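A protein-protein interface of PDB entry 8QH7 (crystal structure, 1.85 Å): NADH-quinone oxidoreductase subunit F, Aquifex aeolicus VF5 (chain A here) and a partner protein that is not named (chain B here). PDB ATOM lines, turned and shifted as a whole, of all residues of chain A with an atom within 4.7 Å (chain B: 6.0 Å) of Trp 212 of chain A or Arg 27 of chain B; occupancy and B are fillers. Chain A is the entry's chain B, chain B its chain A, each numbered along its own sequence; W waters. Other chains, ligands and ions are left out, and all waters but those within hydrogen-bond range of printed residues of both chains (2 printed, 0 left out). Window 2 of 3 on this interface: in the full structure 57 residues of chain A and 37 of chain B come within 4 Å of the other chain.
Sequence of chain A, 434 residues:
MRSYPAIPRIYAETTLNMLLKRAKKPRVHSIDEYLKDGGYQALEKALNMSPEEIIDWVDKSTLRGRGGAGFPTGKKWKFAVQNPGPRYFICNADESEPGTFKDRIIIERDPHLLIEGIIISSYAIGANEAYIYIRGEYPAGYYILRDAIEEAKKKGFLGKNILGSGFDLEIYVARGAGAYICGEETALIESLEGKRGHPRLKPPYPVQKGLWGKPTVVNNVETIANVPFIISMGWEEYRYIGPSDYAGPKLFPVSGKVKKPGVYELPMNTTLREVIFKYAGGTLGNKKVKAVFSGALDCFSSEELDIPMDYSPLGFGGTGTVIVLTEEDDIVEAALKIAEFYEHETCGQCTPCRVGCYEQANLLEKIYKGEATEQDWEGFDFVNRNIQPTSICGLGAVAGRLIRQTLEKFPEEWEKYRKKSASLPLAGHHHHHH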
ATOM      1  N   TYR A  88      16.206   6.785  38.181  1.00  0.00           N
ATOM      2  CA  TYR A  88      15.317   6.947  37.045  1.00  0.00           C
ATOM      3  C   TYR A  88      14.703   5.599  36.680  1.00  0.00           C
ATOM      4  O   TYR A  88      15.328   4.556  36.868  1.00  0.00           O
ATOM      5  CB  TYR A  88      16.084   7.524  35.850  1.00  0.00           C
ATOM      6  CG  TYR A  88      16.688   8.876  36.121  1.00  0.00           C
ATOM      7  CD1 TYR A  88      15.884   9.983  36.317  1.00  0.00           C
ATOM      8  CD2 TYR A  88      18.058   9.044  36.209  1.00  0.00           C
ATOM      9  CE1 TYR A  88      16.431  11.230  36.580  1.00  0.00           C
ATOM     10  CE2 TYR A  88      18.620  10.280  36.485  1.00  0.00           C
ATOM     11  CZ  TYR A  88      17.804  11.379  36.661  1.00  0.00           C
ATOM     12  OH  TYR A  88      18.373  12.603  36.918  1.00  0.00           O
ATOM     13  N   LEU A 192      18.401   8.820  24.993  1.00  0.00           N
ATOM     14  CA  LEU A 192      17.648   9.697  25.876  1.00  0.00           C
ATOM     15  C   LEU A 192      18.486  10.919  26.255  1.00  0.00           C
ATOM     16  O   LEU A 192      17.938  11.968  26.582  1.00  0.00           O
ATOM     17  CB  LEU A 192      17.250   8.933  27.142  1.00  0.00           C
ATOM     18  CG  LEU A 192      15.999   8.072  27.053  1.00  0.00           C
ATOM     19  CD1 LEU A 192      15.752   7.377  28.377  1.00  0.00           C
ATOM     20  CD2 LEU A 192      14.790   8.918  26.661  1.00  0.00           C
ATOM     21  N   GLU A 193      19.815  10.762  26.250  1.00  0.00           N
ATOM     22  CA  GLU A 193      20.723  11.842  26.592  1.00  0.00           C
ATOM     23  C   GLU A 193      21.005  12.735  25.379  1.00  0.00           C
ATOM     24  O   GLU A 193      21.792  13.684  25.478  1.00  0.00           O
ATOM     25  CB  GLU A 193      22.018  11.262  27.172  1.00  0.00           C
ATOM     26  CG  GLU A 193      21.858  10.611  28.539  1.00  0.00           C
ATOM     27  CD  GLU A 193      23.146  10.063  29.145  1.00  0.00           C
ATOM     28  OE1 GLU A 193      23.099   9.569  30.289  1.00  0.00           O
ATOM     29  OE2 GLU A 193      24.211  10.131  28.470  1.00  0.00           O
ATOM     30  N   GLY A 194      20.423  12.404  24.219  1.00  0.00           N
ATOM     31  CA  GLY A 194      20.512  13.262  23.047  1.00  0.00           C
ATOM     32  C   GLY A 194      21.623  12.855  22.080  1.00  0.00           C
ATOM     33  O   GLY A 194      22.012  13.640  21.211  1.00  0.00           O
ATOM     34  N   GLY A 210      23.455   4.765  34.999  1.00  0.00           N
ATOM     35  CA  GLY A 210      22.551   4.807  33.862  1.00  0.00           C
ATOM     36  C   GLY A 210      22.418   6.209  33.276  1.00  0.00           C
ATOM     37  O   GLY A 210      23.411   6.805  32.856  1.00  0.00           O
ATOM     38  N   LEU A 211      21.174   6.710  33.262  1.00  0.00           N
ATOM     39  CA  LEU A 211      20.850   8.029  32.743  1.00  0.00           C
ATOM     40  C   LEU A 211      21.523   9.087  33.609  1.00  0.00           C
ATOM     41  O   LEU A 211      21.305   9.111  34.815  1.00  0.00           O
ATOM     42  CB  LEU A 211      19.327   8.194  32.727  1.00  0.00           C
ATOM     43  CG  LEU A 211      18.817   9.511  32.151  1.00  0.00           C
ATOM     44  CD1 LEU A 211      19.135   9.628  30.671  1.00  0.00           C
ATOM     45  CD2 LEU A 211      17.327   9.677  32.389  1.00  0.00           C
ATOM     46  N   TRP A 212      22.345   9.932  32.969  1.00  0.00           N
ATOM     47  CA  TRP A 212      23.150  10.948  33.631  1.00  0.00           C
ATOM     48  C   TRP A 212      24.025  10.313  34.717  1.00  0.00           C
ATOM     49  O   TRP A 212      24.377  10.966  35.701  1.00  0.00           O
ATOM     50  CB  TRP A 212      22.269  12.072  34.191  1.00  0.00           C
ATOM     51  CG  TRP A 212      21.250  12.603  33.231  1.00  0.00           C
ATOM     52  CD1 TRP A 212      19.911  12.724  33.458  1.00  0.00           C
ATOM     53  CD2 TRP A 212      21.478  13.123  31.907  1.00  0.00           C
ATOM     54  NE1 TRP A 212      19.281  13.236  32.355  1.00  0.00           N
ATOM     55  CE2 TRP A 212      20.217  13.503  31.391  1.00  0.00           C
ATOM     56  CE3 TRP A 212      22.611  13.300  31.107  1.00  0.00           C
ATOM     57  CZ2 TRP A 212      20.062  14.050  30.121  1.00  0.00           C
ATOM     58  CZ3 TRP A 212      22.457  13.831  29.845  1.00  0.00           C
ATOM     59  CH2 TRP A 212      21.197  14.194  29.359  1.00  0.00           C
ATOM     60  N   GLY A 213      24.366   9.031  34.526  1.00  0.00           N
ATOM     61  CA  GLY A 213      25.235   8.303  35.439  1.00  0.00           C
ATOM     62  C   GLY A 213      24.577   7.882  36.758  1.00  0.00           C
ATOM     63  O   GLY A 213      25.273   7.423  37.657  1.00  0.00           O
ATOM     64  N   LYS A 214      23.252   8.025  36.869  1.00  0.00           N
ATOM     65  CA  LYS A 214      22.530   7.728  38.101  1.00  0.00           C
ATOM     66  C   LYS A 214      21.903   6.337  38.019  1.00  0.00           C
ATOM     67  O   LYS A 214      21.702   5.816  36.924  1.00  0.00           O
ATOM     68  CB  LYS A 214      21.433   8.771  38.332  1.00  0.00           C
ATOM     69  CG  LYS A 214      21.905  10.218  38.385  1.00  0.00           C
ATOM     70  CD  LYS A 214      22.984  10.454  39.403  1.00  0.00           C
ATOM     71  CE  LYS A 214      23.363  11.916  39.526  1.00  0.00           C
ATOM     72  NZ  LYS A 214      24.604  12.071  40.314  1.00  0.00           N
ATOM     73  N   LYS B  25      16.262  18.420  30.202  1.00  0.00           N
ATOM     74  CA  LYS B  25      17.428  19.005  29.539  1.00  0.00           C
ATOM     75  C   LYS B  25      17.132  19.208  28.054  1.00  0.00           C
ATOM     76  O   LYS B  25      16.485  18.376  27.425  1.00  0.00           O
ATOM     77  CB  LYS B  25      18.684  18.144  29.731  1.00  0.00           C
ATOM     78  CG  LYS B  25      19.030  17.836  31.184  1.00  0.00           C
ATOM     79  CD  LYS B  25      20.430  17.299  31.393  1.00  0.00           C
ATOM     80  CE  LYS B  25      20.737  16.982  32.843  1.00  0.00           C
ATOM     81  NZ  LYS B  25      22.128  16.492  33.029  1.00  0.00           N
ATOM     82  N   LYS B  26      17.609  20.333  27.506  1.00  0.00           N
ATOM     83  CA  LYS B  26      17.271  20.736  26.149  1.00  0.00           C
ATOM     84  C   LYS B  26      17.695  19.664  25.145  1.00  0.00           C
ATOM     85  O   LYS B  26      16.935  19.333  24.234  1.00  0.00           O
ATOM     86  CB  LYS B  26      17.929  22.071  25.789  1.00  0.00           C
ATOM     87  CG  LYS B  26      17.361  23.290  26.495  1.00  0.00           C
ATOM     88  CD  LYS B  26      17.830  24.595  25.880  1.00  0.00           C
ATOM     89  CE  LYS B  26      17.106  25.811  26.421  1.00  0.00           C
ATOM     90  NZ  LYS B  26      17.862  26.433  27.528  1.00  0.00           N
ATOM     91  N   ARG B  27      18.890  19.090  25.347  1.00  0.00           N
ATOM     92  CA  ARG B  27      19.492  18.213  24.355  1.00  0.00           C
ATOM     93  C   ARG B  27      18.688  16.931  24.158  1.00  0.00           C
ATOM     94  O   ARG B  27      18.825  16.311  23.111  1.00  0.00           O
ATOM     95  CB  ARG B  27      20.952  17.893  24.678  1.00  0.00           C
ATOM     96  CG  ARG B  27      21.206  17.200  26.008  1.00  0.00           C
ATOM     97  CD  ARG B  27      22.659  17.456  26.341  1.00  0.00           C
ATOM     98  NE  ARG B  27      23.143  16.921  27.605  1.00  0.00           N
ATOM     99  CZ  ARG B  27      23.296  17.630  28.714  1.00  0.00           C
ATOM    100  NH1 ARG B  27      24.027  17.161  29.710  1.00  0.00           N
ATOM    101  NH2 ARG B  27      22.760  18.832  28.800  1.00  0.00           N
ATOM    102  N   GLN B  28      17.838  16.556  25.125  1.00  0.00           N
ATOM    103  CA  GLN B  28      17.044  15.337  25.024  1.00  0.00           C
ATOM    104  C   GLN B  28      15.979  15.439  23.923  1.00  0.00           C
ATOM    105  O   GLN B  28      15.469  14.414  23.464  1.00  0.00           O
ATOM    106  CB  GLN B  28      16.362  15.015  26.362  1.00  0.00           C
ATOM    107  CG  GLN B  28      17.296  15.000  27.562  1.00  0.00           C
ATOM    108  CD  GLN B  28      16.618  14.465  28.801  1.00  0.00           C
ATOM    109  OE1 GLN B  28      16.269  15.214  29.717  1.00  0.00           O
ATOM    110  NE2 GLN B  28      16.404  13.158  28.828  1.00  0.00           N
ATOM    111  N   ALA B  29      15.660  16.666  23.474  1.00  0.00           N
ATOM    112  CA  ALA B  29      14.607  16.883  22.487  1.00  0.00           C
ATOM    113  C   ALA B  29      15.094  16.713  21.044  1.00  0.00           C
ATOM    114  O   ALA B  29      14.299  16.897  20.125  1.00  0.00           O
ATOM    115  CB  ALA B  29      14.017  18.258  22.687  1.00  0.00           C
ATOM    116  N   ILE B  30      16.363  16.313  20.838  1.00  0.00           N
ATOM    117  CA  ILE B  30      16.984  16.342  19.519  1.00  0.00           C
ATOM    118  C   ILE B  30      16.184  15.531  18.491  1.00  0.00           C
ATOM    119  O   ILE B  30      15.916  16.045  17.411  1.00  0.00           O
ATOM    120  CB  ILE B  30      18.476  15.940  19.564  1.00  0.00           C
ATOM    121  CG1 ILE B  30      19.140  16.119  18.196  1.00  0.00           C
ATOM    122  CG2 ILE B  30      18.673  14.531  20.105  1.00  0.00           C
ATOM    123  CD1 ILE B  30      20.651  16.119  18.251  1.00  0.00           C
ATOM    124  N   LEU B  31      15.767  14.301  18.816  1.00  0.00           N
ATOM    125  CA  LEU B  31      15.045  13.464  17.863  1.00  0.00           C
ATOM    126  C   LEU B  31      13.628  13.987  17.604  1.00  0.00           C
ATOM    127  O   LEU B  31      13.155  13.938  16.469  1.00  0.00           O
ATOM    128  CB  LEU B  31      15.011  12.020  18.376  1.00  0.00           C
ATOM    129  CG  LEU B  31      16.379  11.378  18.608  1.00  0.00           C
ATOM    130  CD1 LEU B  31      16.257   9.910  18.950  1.00  0.00           C
ATOM    131  CD2 LEU B  31      17.269  11.567  17.394  1.00  0.00           C
ATOM    132  N   LEU B  56      19.321  23.802  20.645  1.00  0.00           N
ATOM    133  CA  LEU B  56      19.595  22.689  21.546  1.00  0.00           C
ATOM    134  C   LEU B  56      20.834  22.941  22.412  1.00  0.00           C
ATOM    135  O   LEU B  56      21.103  22.172  23.333  1.00  0.00           O
ATOM    136  CB  LEU B  56      19.814  21.424  20.701  1.00  0.00           C
ATOM    137  CG  LEU B  56      18.602  20.887  19.943  1.00  0.00           C
ATOM    138  CD1 LEU B  56      19.011  19.754  19.009  1.00  0.00           C
ATOM    139  CD2 LEU B  56      17.524  20.410  20.904  1.00  0.00           C
ATOM    140  N   LEU B  58      23.853  22.562  21.405  1.00  0.00           N
ATOM    141  CA  LEU B  58      24.769  21.491  21.043  1.00  0.00           C
ATOM    142  C   LEU B  58      25.676  21.985  19.921  1.00  0.00           C
ATOM    143  O   LEU B  58      25.282  22.867  19.160  1.00  0.00           O
ATOM    144  CB  LEU B  58      23.968  20.277  20.571  1.00  0.00           C
ATOM    145  CG  LEU B  58      23.258  19.469  21.657  1.00  0.00           C
ATOM    146  CD1 LEU B  58      22.430  18.347  21.042  1.00  0.00           C
ATOM    147  CD2 LEU B  58      24.257  18.916  22.664  1.00  0.00           C
ATOM    148  N   HIS B  62      27.719  17.477  16.426  1.00  0.00           N
ATOM    149  CA  HIS B  62      26.889  16.577  17.220  1.00  0.00           C
ATOM    150  C   HIS B  62      25.571  16.313  16.496  1.00  0.00           C
ATOM    151  O   HIS B  62      25.182  15.161  16.307  1.00  0.00           O
ATOM    152  CB  HIS B  62      26.629  17.154  18.617  1.00  0.00           C
ATOM    153  CG  HIS B  62      25.811  16.285  19.523  1.00  0.00           C
ATOM    154  ND1 HIS B  62      26.156  16.116  20.846  1.00  0.00           N
ATOM    155  CD2 HIS B  62      24.678  15.589  19.350  1.00  0.00           C
ATOM    156  CE1 HIS B  62      25.266  15.330  21.433  1.00  0.00           C
ATOM    157  NE2 HIS B  62      24.368  14.989  20.541  1.00  0.00           N
HETATM  158  O   HOH W   1      24.316  14.296  26.693  1.00  0.00           O
HETATM  159  O   HOH W   2      16.649  14.555  32.379  1.00  0.00           O
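N of Lys 25 of chain B is in hydrogen-bond range of OE1 of Gln 28 of chain B (3.2 Å). The side-chain carboxylate of Glu 193 of chain A sits at hydrogen-bond distance from the backbone NH of Trp 212 of chain A, at 2.8 Å.
Arg 27 of chain B touches Glu 193 of chain A (CG to O, 3.6 Å). Gly 194 of chain A touches Arg 27 of chain B. O of Gly 194 of chain A touches CG2 of Ile 30 of chain B (3.6 Å). CD of Lys 25 of chain B touches CZ2 of Trp 212 of chain A, 3.5 Å away. Arg 27 of chain B touches Trp 212 of chain A (NH1 to CZ3, 3.7 Å). CD of Gln 28 of chain B touches CZ2 of Trp 212 of chain A (3.7 Å).
Of the printed residues of chain B, Glu 193 of chain A touches Arg 27. Of chain B, only Lys 25 (3.5 Å), Arg 27 (3.7 Å) and Gln 28 (3.7 Å) come within 4 Å of Trp 212 of chain A. Printed residues of chain A within 4 Å of Ile 30 of chain B: Gly 194. Leu 56 of chain B touches none of the printed residues of chain A. Of the printed residues of chain A, His 62 of chain B touches Gly 194. The nearest printed residue of chain B that does not touch Trp 212 of chain A is Lys 26 of chain B (7.2 Å).
Printed residues of chain A that touch a printed residue of chain B: Leu 192, Glu 193, Gly 194 and Trp 212. Hydrophobic or aromatic side chains of chain A that line the printed part of chain B: Trp 212. Hydrophobic or aromatic side chains of chain B within 4 Å of the printed part of chain A: Ile 30 and His 62.
NE2 of His 62 of chain B is in hydrogen-bond range of O of Gly 194 of chain A (2.8 Å). The side-chain amide nitrogen (NE2) of Gln 28 of chain B sits at hydrogen-bond distance from the backbone carbonyl oxygen (O) of Leu 192 of chain A (3.0 Å).
Water W2 bridges the side-chain amide oxygen (OE1) of Gln 28 of chain B (2.8 Å) and the indole nitrogen (NE1) of Trp 212 of chain A (2.9 Å). Water W1 lies within hydrogen-bond range of O of Glu 193 of chain A and NE of Arg 27 of chain B.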
